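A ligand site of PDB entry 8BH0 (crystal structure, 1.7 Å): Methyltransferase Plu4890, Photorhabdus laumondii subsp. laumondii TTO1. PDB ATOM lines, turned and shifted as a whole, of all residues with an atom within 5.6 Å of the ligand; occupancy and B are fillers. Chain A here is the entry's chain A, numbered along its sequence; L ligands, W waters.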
ATOM      1  N   PHE A 127      23.633  -5.293  26.394  1.00  0.00           N
ATOM      2  CA  PHE A 127      23.388  -5.957  25.090  1.00  0.00           C
ATOM      3  C   PHE A 127      23.465  -7.484  25.242  1.00  0.00           C
ATOM      4  O   PHE A 127      22.680  -8.180  24.572  1.00  0.00           O
ATOM      5  CB  PHE A 127      24.304  -5.391  24.002  1.00  0.00           C
ATOM      6  CG  PHE A 127      23.908  -3.993  23.584  1.00  0.00           C
ATOM      7  CD1 PHE A 127      22.651  -3.750  23.052  1.00  0.00           C
ATOM      8  CD2 PHE A 127      24.779  -2.919  23.739  1.00  0.00           C
ATOM      9  CE1 PHE A 127      22.270  -2.475  22.684  1.00  0.00           C
ATOM     10  CE2 PHE A 127      24.399  -1.640  23.358  1.00  0.00           C
ATOM     11  CZ  PHE A 127      23.138  -1.424  22.839  1.00  0.00           C
ATOM     12  N   LYS A 137      14.767  -6.296  24.404  1.00  0.00           N
ATOM     13  CA  LYS A 137      15.381  -6.341  23.053  1.00  0.00           C
ATOM     14  C   LYS A 137      14.383  -5.795  22.018  1.00  0.00           C
ATOM     15  O   LYS A 137      14.782  -4.940  21.217  1.00  0.00           O
ATOM     16  CB  LYS A 137      15.843  -7.751  22.678  1.00  0.00           C
ATOM     17  CG  LYS A 137      16.347  -7.879  21.239  1.00  0.00           C
ATOM     18  CD  LYS A 137      17.411  -8.933  21.034  1.00  0.00           C
ATOM     19  CE  LYS A 137      18.129  -8.804  19.703  1.00  0.00           C
ATOM     20  NZ  LYS A 137      19.045  -7.642  19.684  1.00  0.00           N
ATOM     21  N   PHE A 140      13.691  -1.945  22.789  1.00  0.00           N
ATOM     22  CA  PHE A 140      14.929  -1.155  22.534  1.00  0.00           C
ATOM     23  C   PHE A 140      15.157  -1.068  21.020  1.00  0.00           C
ATOM     24  O   PHE A 140      15.370   0.038  20.499  1.00  0.00           O
ATOM     25  CB  PHE A 140      16.146  -1.760  23.231  1.00  0.00           C
ATOM     26  CG  PHE A 140      17.411  -0.968  23.010  1.00  0.00           C
ATOM     27  CD1 PHE A 140      17.748   0.089  23.859  1.00  0.00           C
ATOM     28  CD2 PHE A 140      18.248  -1.244  21.941  1.00  0.00           C
ATOM     29  CE1 PHE A 140      18.896   0.833  23.644  1.00  0.00           C
ATOM     30  CE2 PHE A 140      19.397  -0.500  21.727  1.00  0.00           C
ATOM     31  CZ  PHE A 140      19.721   0.540  22.583  1.00  0.00           C
ATOM     32  N   ASP A 141      15.120  -2.213  20.331  1.00  0.00           N
ATOM     33  CA  ASP A 141      15.349  -2.285  18.862  1.00  0.00           C
ATOM     34  C   ASP A 141      14.263  -1.493  18.125  1.00  0.00           C
ATOM     35  O   ASP A 141      14.604  -0.818  17.142  1.00  0.00           O
ATOM     36  CB  ASP A 141      15.445  -3.741  18.378  1.00  0.00           C
ATOM     37  CG  ASP A 141      16.775  -4.409  18.699  1.00  0.00           C
ATOM     38  OD1 ASP A 141      17.643  -3.742  19.310  1.00  0.00           O
ATOM     39  OD2 ASP A 141      16.936  -5.586  18.327  1.00  0.00           O
ATOM     40  N   MET A 144      15.106   2.300  18.526  1.00  0.00           N
ATOM     41  CA  MET A 144      16.246   2.650  17.634  1.00  0.00           C
ATOM     42  C   MET A 144      15.742   2.748  16.187  1.00  0.00           C
ATOM     43  O   MET A 144      16.170   3.690  15.480  1.00  0.00           O
ATOM     44  CB  MET A 144      17.361   1.596  17.721  1.00  0.00           C
ATOM     45  CG  MET A 144      18.071   1.549  19.076  1.00  0.00           C
ATOM     46  SD  MET A 144      18.728   3.143  19.622  1.00  0.00           S
ATOM     47  CE  MET A 144      17.570   3.574  20.921  1.00  0.00           C
ATOM     48  N   THR A 145      14.862   1.841  15.771  1.00  0.00           N
ATOM     49  CA  THR A 145      14.238   1.819  14.410  1.00  0.00           C
ATOM     50  C   THR A 145      13.471   3.131  14.193  1.00  0.00           C
ATOM     51  O   THR A 145      13.654   3.754  13.127  1.00  0.00           O
ATOM     52  CB  THR A 145      13.375   0.570  14.219  1.00  0.00           C
ATOM     53  OG1 THR A 145      14.252  -0.540  14.120  1.00  0.00           O
ATOM     54  CG2 THR A 145      12.472   0.633  13.002  1.00  0.00           C
ATOM     55  N   VAL A 147      13.713   6.140  15.762  1.00  0.00           N
ATOM     56  CA  VAL A 147      14.600   7.339  15.767  1.00  0.00           C
ATOM     57  C   VAL A 147      15.444   7.349  14.480  1.00  0.00           C
ATOM     58  O   VAL A 147      15.755   8.460  13.995  1.00  0.00           O
ATOM     59  CB  VAL A 147      15.463   7.441  17.035  1.00  0.00           C
ATOM     60  CG1 VAL A 147      14.604   7.559  18.281  1.00  0.00           C
ATOM     61  CG2 VAL A 147      16.443   6.286  17.175  1.00  0.00           C
ATOM     62  N   SER A 148      15.803   6.179  13.947  1.00  0.00           N
ATOM     63  CA  SER A 148      16.494   6.033  12.640  1.00  0.00           C
ATOM     64  C   SER A 148      15.583   6.558  11.519  1.00  0.00           C
ATOM     65  O   SER A 148      16.069   7.330  10.686  1.00  0.00           O
ATOM     66  CB  SER A 148      16.903   4.607  12.380  1.00  0.00           C
ATOM     67  OG  SER A 148      17.917   4.197  13.283  1.00  0.00           O
ATOM     68  N   ASP A 169      26.299  -0.627   7.302  1.00  0.00           N
ATOM     69  CA  ASP A 169      25.829   0.017   8.566  1.00  0.00           C
ATOM     70  C   ASP A 169      26.235  -0.894   9.739  1.00  0.00           C
ATOM     71  O   ASP A 169      25.660  -1.993   9.846  1.00  0.00           O
ATOM     72  CB  ASP A 169      24.333   0.292   8.541  1.00  0.00           C
ATOM     73  CG  ASP A 169      23.885   1.287   9.612  1.00  0.00           C
ATOM     74  OD1 ASP A 169      24.773   1.934  10.211  1.00  0.00           O
ATOM     75  OD2 ASP A 169      22.675   1.411   9.821  1.00  0.00           O
ATOM     76  N   VAL A 170      27.175  -0.434  10.567  1.00  0.00           N
ATOM     77  CA  VAL A 170      27.779  -1.223  11.679  1.00  0.00           C
ATOM     78  C   VAL A 170      27.013  -0.930  12.966  1.00  0.00           C
ATOM     79  O   VAL A 170      26.877   0.262  13.310  1.00  0.00           O
ATOM     80  CB  VAL A 170      29.279  -0.912  11.807  1.00  0.00           C
ATOM     81  CG1 VAL A 170      29.885  -1.528  13.068  1.00  0.00           C
ATOM     82  CG2 VAL A 170      30.056  -1.359  10.573  1.00  0.00           C
ATOM     83  N   GLY A 171      26.537  -1.980  13.645  1.00  0.00           N
ATOM     84  CA  GLY A 171      25.579  -1.878  14.760  1.00  0.00           C
ATOM     85  C   GLY A 171      24.257  -1.285  14.286  1.00  0.00           C
ATOM     86  O   GLY A 171      23.674  -0.479  15.019  1.00  0.00           O
ATOM     87  N   GLY A 172      23.804  -1.689  13.088  1.00  0.00           N
ATOM     88  CA  GLY A 172      22.620  -1.119  12.421  1.00  0.00           C
ATOM     89  C   GLY A 172      21.307  -1.686  12.930  1.00  0.00           C
ATOM     90  O   GLY A 172      20.248  -1.215  12.442  1.00  0.00           O
ATOM     91  N   GLY A 173      21.339  -2.658  13.845  1.00  0.00           N
ATOM     92  CA  GLY A 173      20.152  -3.243  14.493  1.00  0.00           C
ATOM     93  C   GLY A 173      19.233  -3.909  13.476  1.00  0.00           C
ATOM     94  O   GLY A 173      19.696  -4.803  12.758  1.00  0.00           O
ATOM     95  N   LEU A 193      25.616  -4.908   9.826  1.00  0.00           N
ATOM     96  CA  LEU A 193      26.341  -5.742  10.810  1.00  0.00           C
ATOM     97  C   LEU A 193      25.775  -5.460  12.202  1.00  0.00           C
ATOM     98  O   LEU A 193      25.676  -4.271  12.572  1.00  0.00           O
ATOM     99  CB  LEU A 193      27.847  -5.460  10.741  1.00  0.00           C
ATOM    100  CG  LEU A 193      28.717  -6.373  11.604  1.00  0.00           C
ATOM    101  CD1 LEU A 193      30.104  -6.534  10.999  1.00  0.00           C
ATOM    102  CD2 LEU A 193      28.815  -5.863  13.032  1.00  0.00           C
ATOM    103  N   ASP A 194      25.415  -6.511  12.934  1.00  0.00           N
ATOM    104  CA  ASP A 194      25.000  -6.427  14.354  1.00  0.00           C
ATOM    105  C   ASP A 194      25.185  -7.809  14.976  1.00  0.00           C
ATOM    106  O   ASP A 194      25.755  -8.695  14.304  1.00  0.00           O
ATOM    107  CB  ASP A 194      23.563  -5.900  14.475  1.00  0.00           C
ATOM    108  CG  ASP A 194      23.297  -5.122  15.751  1.00  0.00           C
ATOM    109  OD1 ASP A 194      23.335  -5.734  16.835  1.00  0.00           O
ATOM    110  OD2 ASP A 194      23.056  -3.895  15.649  1.00  0.00           O
ATOM    111  N   ARG A 195      24.724  -7.983  16.219  1.00  0.00           N
ATOM    112  CA  ARG A 195      24.756  -9.272  16.943  1.00  0.00           C
ATOM    113  C   ARG A 195      23.413  -9.991  16.689  1.00  0.00           C
ATOM    114  O   ARG A 195      22.401  -9.590  17.296  1.00  0.00           O
ATOM    115  CB  ARG A 195      25.036  -9.018  18.428  1.00  0.00           C
ATOM    116  CG  ARG A 195      26.385  -8.348  18.673  1.00  0.00           C
ATOM    117  CD  ARG A 195      26.659  -8.084  20.131  1.00  0.00           C
ATOM    118  NE  ARG A 195      26.741  -9.320  20.910  1.00  0.00           N
ATOM    119  CZ  ARG A 195      25.772  -9.805  21.688  1.00  0.00           C
ATOM    120  NH1 ARG A 195      24.626  -9.161  21.834  1.00  0.00           N
ATOM    121  NH2 ARG A 195      25.977 -10.942  22.335  1.00  0.00           N
ATOM    122  N   GLY A 210      28.139 -10.107  13.485  1.00  0.00           N
ATOM    123  CA  GLY A 210      29.502  -9.609  13.727  1.00  0.00           C
ATOM    124  C   GLY A 210      29.676  -9.066  15.131  1.00  0.00           C
ATOM    125  O   GLY A 210      28.722  -9.135  15.939  1.00  0.00           O
ATOM    126  N   ASN A 211      30.875  -8.558  15.415  1.00  0.00           N
ATOM    127  CA  ASN A 211      31.273  -7.980  16.725  1.00  0.00           C
ATOM    128  C   ASN A 211      32.290  -6.869  16.445  1.00  0.00           C
ATOM    129  O   ASN A 211      33.457  -7.208  16.173  1.00  0.00           O
ATOM    130  CB  ASN A 211      31.808  -9.057  17.662  1.00  0.00           C
ATOM    131  CG  ASN A 211      32.229  -8.522  19.005  1.00  0.00           C
ATOM    132  OD1 ASN A 211      32.101  -7.324  19.269  1.00  0.00           O
ATOM    133  ND2 ASN A 211      32.730  -9.392  19.872  1.00  0.00           N
ATOM    134  N   PHE A 212      31.875  -5.597  16.523  1.00  0.00           N
ATOM    135  CA  PHE A 212      32.706  -4.441  16.122  1.00  0.00           C
ATOM    136  C   PHE A 212      33.849  -4.213  17.131  1.00  0.00           C
ATOM    137  O   PHE A 212      34.759  -3.428  16.817  1.00  0.00           O
ATOM    138  CB  PHE A 212      31.868  -3.176  15.880  1.00  0.00           C
ATOM    139  CG  PHE A 212      30.892  -2.758  16.950  1.00  0.00           C
ATOM    140  CD1 PHE A 212      29.596  -2.407  16.607  1.00  0.00           C
ATOM    141  CD2 PHE A 212      31.274  -2.672  18.278  1.00  0.00           C
ATOM    142  CE1 PHE A 212      28.691  -1.993  17.571  1.00  0.00           C
ATOM    143  CE2 PHE A 212      30.368  -2.268  19.246  1.00  0.00           C
ATOM    144  CZ  PHE A 212      29.080  -1.931  18.900  1.00  0.00           C
ATOM    145  N   LEU A 213      33.824  -4.892  18.289  1.00  0.00           N
ATOM    146  CA  LEU A 213      34.938  -4.886  19.272  1.00  0.00           C
ATOM    147  C   LEU A 213      36.085  -5.777  18.778  1.00  0.00           C
ATOM    148  O   LEU A 213      37.251  -5.528  19.165  1.00  0.00           O
ATOM    149  CB  LEU A 213      34.426  -5.375  20.634  1.00  0.00           C
ATOM    150  CG  LEU A 213      33.309  -4.543  21.269  1.00  0.00           C
ATOM    151  CD1 LEU A 213      32.821  -5.187  22.552  1.00  0.00           C
ATOM    152  CD2 LEU A 213      33.777  -3.112  21.539  1.00  0.00           C
ATOM    153  N   LYS A 226      26.127   4.808  13.580  1.00  0.00           N
ATOM    154  CA  LYS A 226      25.114   5.759  14.096  1.00  0.00           C
ATOM    155  C   LYS A 226      24.675   5.347  15.501  1.00  0.00           C
ATOM    156  O   LYS A 226      24.259   4.187  15.669  1.00  0.00           O
ATOM    157  CB  LYS A 226      23.891   5.842  13.175  1.00  0.00           C
ATOM    158  CG  LYS A 226      22.895   6.933  13.545  1.00  0.00           C
ATOM    159  CD  LYS A 226      21.865   7.225  12.487  1.00  0.00           C
ATOM    160  CE  LYS A 226      20.770   6.180  12.395  1.00  0.00           C
ATOM    161  NZ  LYS A 226      19.957   6.132  13.635  1.00  0.00           N
ATOM    162  N   ASN A 227      24.777   6.276  16.456  1.00  0.00           N
ATOM    163  CA  ASN A 227      24.255   6.146  17.841  1.00  0.00           C
ATOM    164  C   ASN A 227      24.799   4.866  18.500  1.00  0.00           C
ATOM    165  O   ASN A 227      24.031   4.206  19.229  1.00  0.00           O
ATOM    166  CB  ASN A 227      22.723   6.176  17.856  1.00  0.00           C
ATOM    167  CG  ASN A 227      22.162   7.551  17.552  1.00  0.00           C
ATOM    168  OD1 ASN A 227      22.829   8.561  17.772  1.00  0.00           O
ATOM    169  ND2 ASN A 227      20.947   7.606  17.036  1.00  0.00           N
ATOM    170  N   VAL A 228      26.077   4.592  18.279  1.00  0.00           N
ATOM    171  CA  VAL A 228      26.746   3.426  18.909  1.00  0.00           C
ATOM    172  C   VAL A 228      27.717   3.871  20.015  1.00  0.00           C
ATOM    173  O   VAL A 228      27.653   3.344  21.084  1.00  0.00           O
ATOM    174  CB  VAL A 228      27.510   2.600  17.862  1.00  0.00           C
ATOM    175  CG1 VAL A 228      28.513   1.683  18.500  1.00  0.00           C
ATOM    176  CG2 VAL A 228      26.575   1.854  16.929  1.00  0.00           C
ATOM    177  N   ASN A 231      27.130   4.226  23.936  1.00  0.00           N
ATOM    178  CA  ASN A 231      26.969   3.003  24.740  1.00  0.00           C
ATOM    179  C   ASN A 231      28.339   2.504  25.215  1.00  0.00           C
ATOM    180  O   ASN A 231      28.378   1.472  25.802  1.00  0.00           O
ATOM    181  CB  ASN A 231      26.343   1.877  23.899  1.00  0.00           C
ATOM    182  CG  ASN A 231      25.041   2.225  23.201  1.00  0.00           C
ATOM    183  OD1 ASN A 231      24.315   3.106  23.610  1.00  0.00           O
ATOM    184  ND2 ASN A 231      24.735   1.504  22.155  1.00  0.00           N
ATOM    185  N   TRP A 232      29.431   3.227  24.941  1.00  0.00           N
ATOM    186  CA  TRP A 232      30.811   2.694  25.187  1.00  0.00           C
ATOM    187  C   TRP A 232      31.694   3.731  25.896  1.00  0.00           C
ATOM    188  O   TRP A 232      31.459   4.945  25.722  1.00  0.00           O
ATOM    189  CB  TRP A 232      31.442   2.221  23.881  1.00  0.00           C
ATOM    190  CG  TRP A 232      30.641   1.139  23.220  1.00  0.00           C
ATOM    191  CD1 TRP A 232      29.759   1.297  22.181  1.00  0.00           C
ATOM    192  CD2 TRP A 232      30.589  -0.249  23.576  1.00  0.00           C
ATOM    193  NE1 TRP A 232      29.186   0.105  21.866  1.00  0.00           N
ATOM    194  CE2 TRP A 232      29.681  -0.872  22.696  1.00  0.00           C
ATOM    195  CE3 TRP A 232      31.239  -1.035  24.544  1.00  0.00           C
ATOM    196  CZ2 TRP A 232      29.388  -2.235  22.758  1.00  0.00           C
ATOM    197  CZ3 TRP A 232      30.959  -2.381  24.598  1.00  0.00           C
ATOM    198  CH2 TRP A 232      30.043  -2.968  23.722  1.00  0.00           C
HETATM  199  N1  LIG L   1      22.737   2.094  14.630  1.00  0.00           N
HETATM  200  C1  LIG L   1      21.328   1.851  15.087  1.00  0.00           C
HETATM  201  C2  LIG L   1      21.290   1.135  16.441  1.00  0.00           C
HETATM  202  C3  LIG L   1      22.103   1.818  17.532  1.00  0.00           C
HETATM  203  S1  LIG L   1      21.862   1.061  19.162  1.00  0.00           S
HETATM  204  C4  LIG L   1      20.591   3.191  15.214  1.00  0.00           C
HETATM  205  O1  LIG L   1      19.365   3.223  15.390  1.00  0.00           O
HETATM  206  O2  LIG L   1      21.208   4.255  15.160  1.00  0.00           O
HETATM  207  C5  LIG L   1      23.392   0.126  19.358  1.00  0.00           C
HETATM  208  C6  LIG L   1      23.475  -1.113  18.488  1.00  0.00           C
HETATM  209  O3  LIG L   1      24.774  -1.727  18.658  1.00  0.00           O
HETATM  210  C7  LIG L   1      22.446  -2.206  18.802  1.00  0.00           C
HETATM  211  O4  LIG L   1      21.782  -2.591  17.606  1.00  0.00           O
HETATM  212  C8  LIG L   1      23.283  -3.341  19.382  1.00  0.00           C
HETATM  213  O5  LIG L   1      22.735  -4.622  19.145  1.00  0.00           O
HETATM  214  C9  LIG L   1      24.597  -3.121  18.642  1.00  0.00           C
HETATM  215  N2  LIG L   1      25.774  -3.739  19.232  1.00  0.00           N
HETATM  216  C10 LIG L   1      26.124  -3.772  20.561  1.00  0.00           C
HETATM  217  N3  LIG L   1      27.257  -4.385  20.777  1.00  0.00           N
HETATM  218  C11 LIG L   1      27.688  -4.782  19.524  1.00  0.00           C
HETATM  219  C12 LIG L   1      28.839  -5.468  19.086  1.00  0.00           C
HETATM  220  N4  LIG L   1      29.798  -5.899  19.906  1.00  0.00           N
HETATM  221  N5  LIG L   1      28.969  -5.690  17.763  1.00  0.00           N
HETATM  222  C13 LIG L   1      28.000  -5.258  16.941  1.00  0.00           C
HETATM  223  N6  LIG L   1      26.881  -4.600  17.238  1.00  0.00           N
HETATM  224  C14 LIG L   1      26.780  -4.386  18.555  1.00  0.00           C
HETATM  225  O   HOH W   1      18.202   1.021  14.390  1.00  0.00           O
HETATM  226  O   HOH W   2      18.980  -1.688  17.693  1.00  0.00           O
HETATM  227  O   HOH W   3      21.945   3.677  21.261  1.00  0.00           O
HETATM  228  O   HOH W   4      25.120   2.240  12.701  1.00  0.00           O
HETATM  229  O   HOH W   5      26.434  -0.255  20.791  1.00  0.00           O
HETATM  230  O   HOH W   6      23.361  -6.857  20.746  1.00  0.00           O
HETATM  231  O   HOH W   7      27.789  -5.869  23.208  1.00  0.00           O
HETATM  232  O   HOH W   8      22.067   2.644  11.915  1.00  0.00           O
HETATM  233  O   HOH W   9      19.369   5.276  17.159  1.00  0.00           O
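The backbone carbonyl oxygen of Met 144 sits close to an oxygen (O1) of the ligand.
Phe 127 touches the ligand.
Phe 140 touches the ligand.
Gly 172 touches the ligand (CA to N1, 3.9 Å).
Gly 173 touches the ligand (CA to O4, 3.6 Å).
Arg 195 touches the ligand (CD to C11, 3.5 Å).
Gly 210 touches the ligand (O to N5, 3.9 Å).
Asn 227 touches the ligand (O to C3, 3.5 Å).
Asn 231 touches the ligand.
Trp 232 touches the ligand (CZ2 to N3, 3.6 Å).
Water W1 lies within hydrogen-bond range of an oxygen (O1) of the ligand (2.7 Å) and the side-chain hydroxyl of Ser 148 (3.4 Å).
Water W9 lies within hydrogen-bond range of O1 of the ligand, ND2 of Asn 227 and SD of Met 144.
Water W6 bridges an oxygen (O5) of the ligand and the guanidinium group (NH1) of Arg 195.
Water W8 lies within hydrogen-bond range of OD2 of Asp 169 and N1 of the ligand.
Water W4 lies within hydrogen-bond range of the side-chain carboxylate of Asp 169 (2.5 Å), the backbone carbonyl oxygen of Val 170 (2.7 Å), the backbone NH of Lys 226 (2.9 Å) and a nitrogen (N1) of the ligand (3.1 Å).
Water W5 lies within hydrogen-bond range of ND2 of Asn 231 (2.8 Å), NE1 of Trp 232 (3.0 Å) and O3 of the ligand (3.1 Å).
The backbone NH of Gly 173 sits at hydrogen-bond distance from the side-chain carboxylate of Asp 194.
N of Gly 171 sits at hydrogen-bond distance from O of Leu 193 (2.7 Å).
NZ of Lys 226 is in hydrogen-bond range of OG of Ser 148 (2.8 Å).
The backbone carbonyl oxygen (O) of Asp 194 sits at hydrogen-bond distance from the backbone NH (N) of Gly 210 (2.9 Å).
The backbone NH of Leu 213 sits close to the side-chain amide oxygen of Asn 211 (3.1 Å).
N of Gly 172 sits at hydrogen-bond distance from O of Leu 193 (3.2 Å).
The backbone carbonyl oxygen (O) of Phe 127 is in hydrogen-bond range of the guanidinium group (NH1) of Arg 195 (3.5 Å).
O of Met 144 is in hydrogen-bond range of OG of Ser 148 (2.9 Å).
The side-chain carboxylate of Asp 194 is in hydrogen-bond range of an oxygen (O5) of the ligand (2.6 Å).
An oxygen (O1) of the ligand sits at hydrogen-bond distance from the side-chain hydroxyl of Ser 148 (2.7 Å).
The backbone carbonyl oxygen of Lys 226 is in hydrogen-bond range of a nitrogen (N1) of the ligand (2.8 Å).
A nitrogen (N4) of the ligand lies within hydrogen-bond range of the side-chain amide oxygen (OD1) of Asn 211 (2.8 Å).
The backbone NH (N) of Phe 212 lies within hydrogen-bond range of a nitrogen (N5) of the ligand.
The backbone carbonyl oxygen (O) of Gly 171 is in hydrogen-bond range of a nitrogen (N1) of the ligand, at 2.8 Å.
O2 of the ligand lies within salt-bridge range of NZ of Lys 226.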
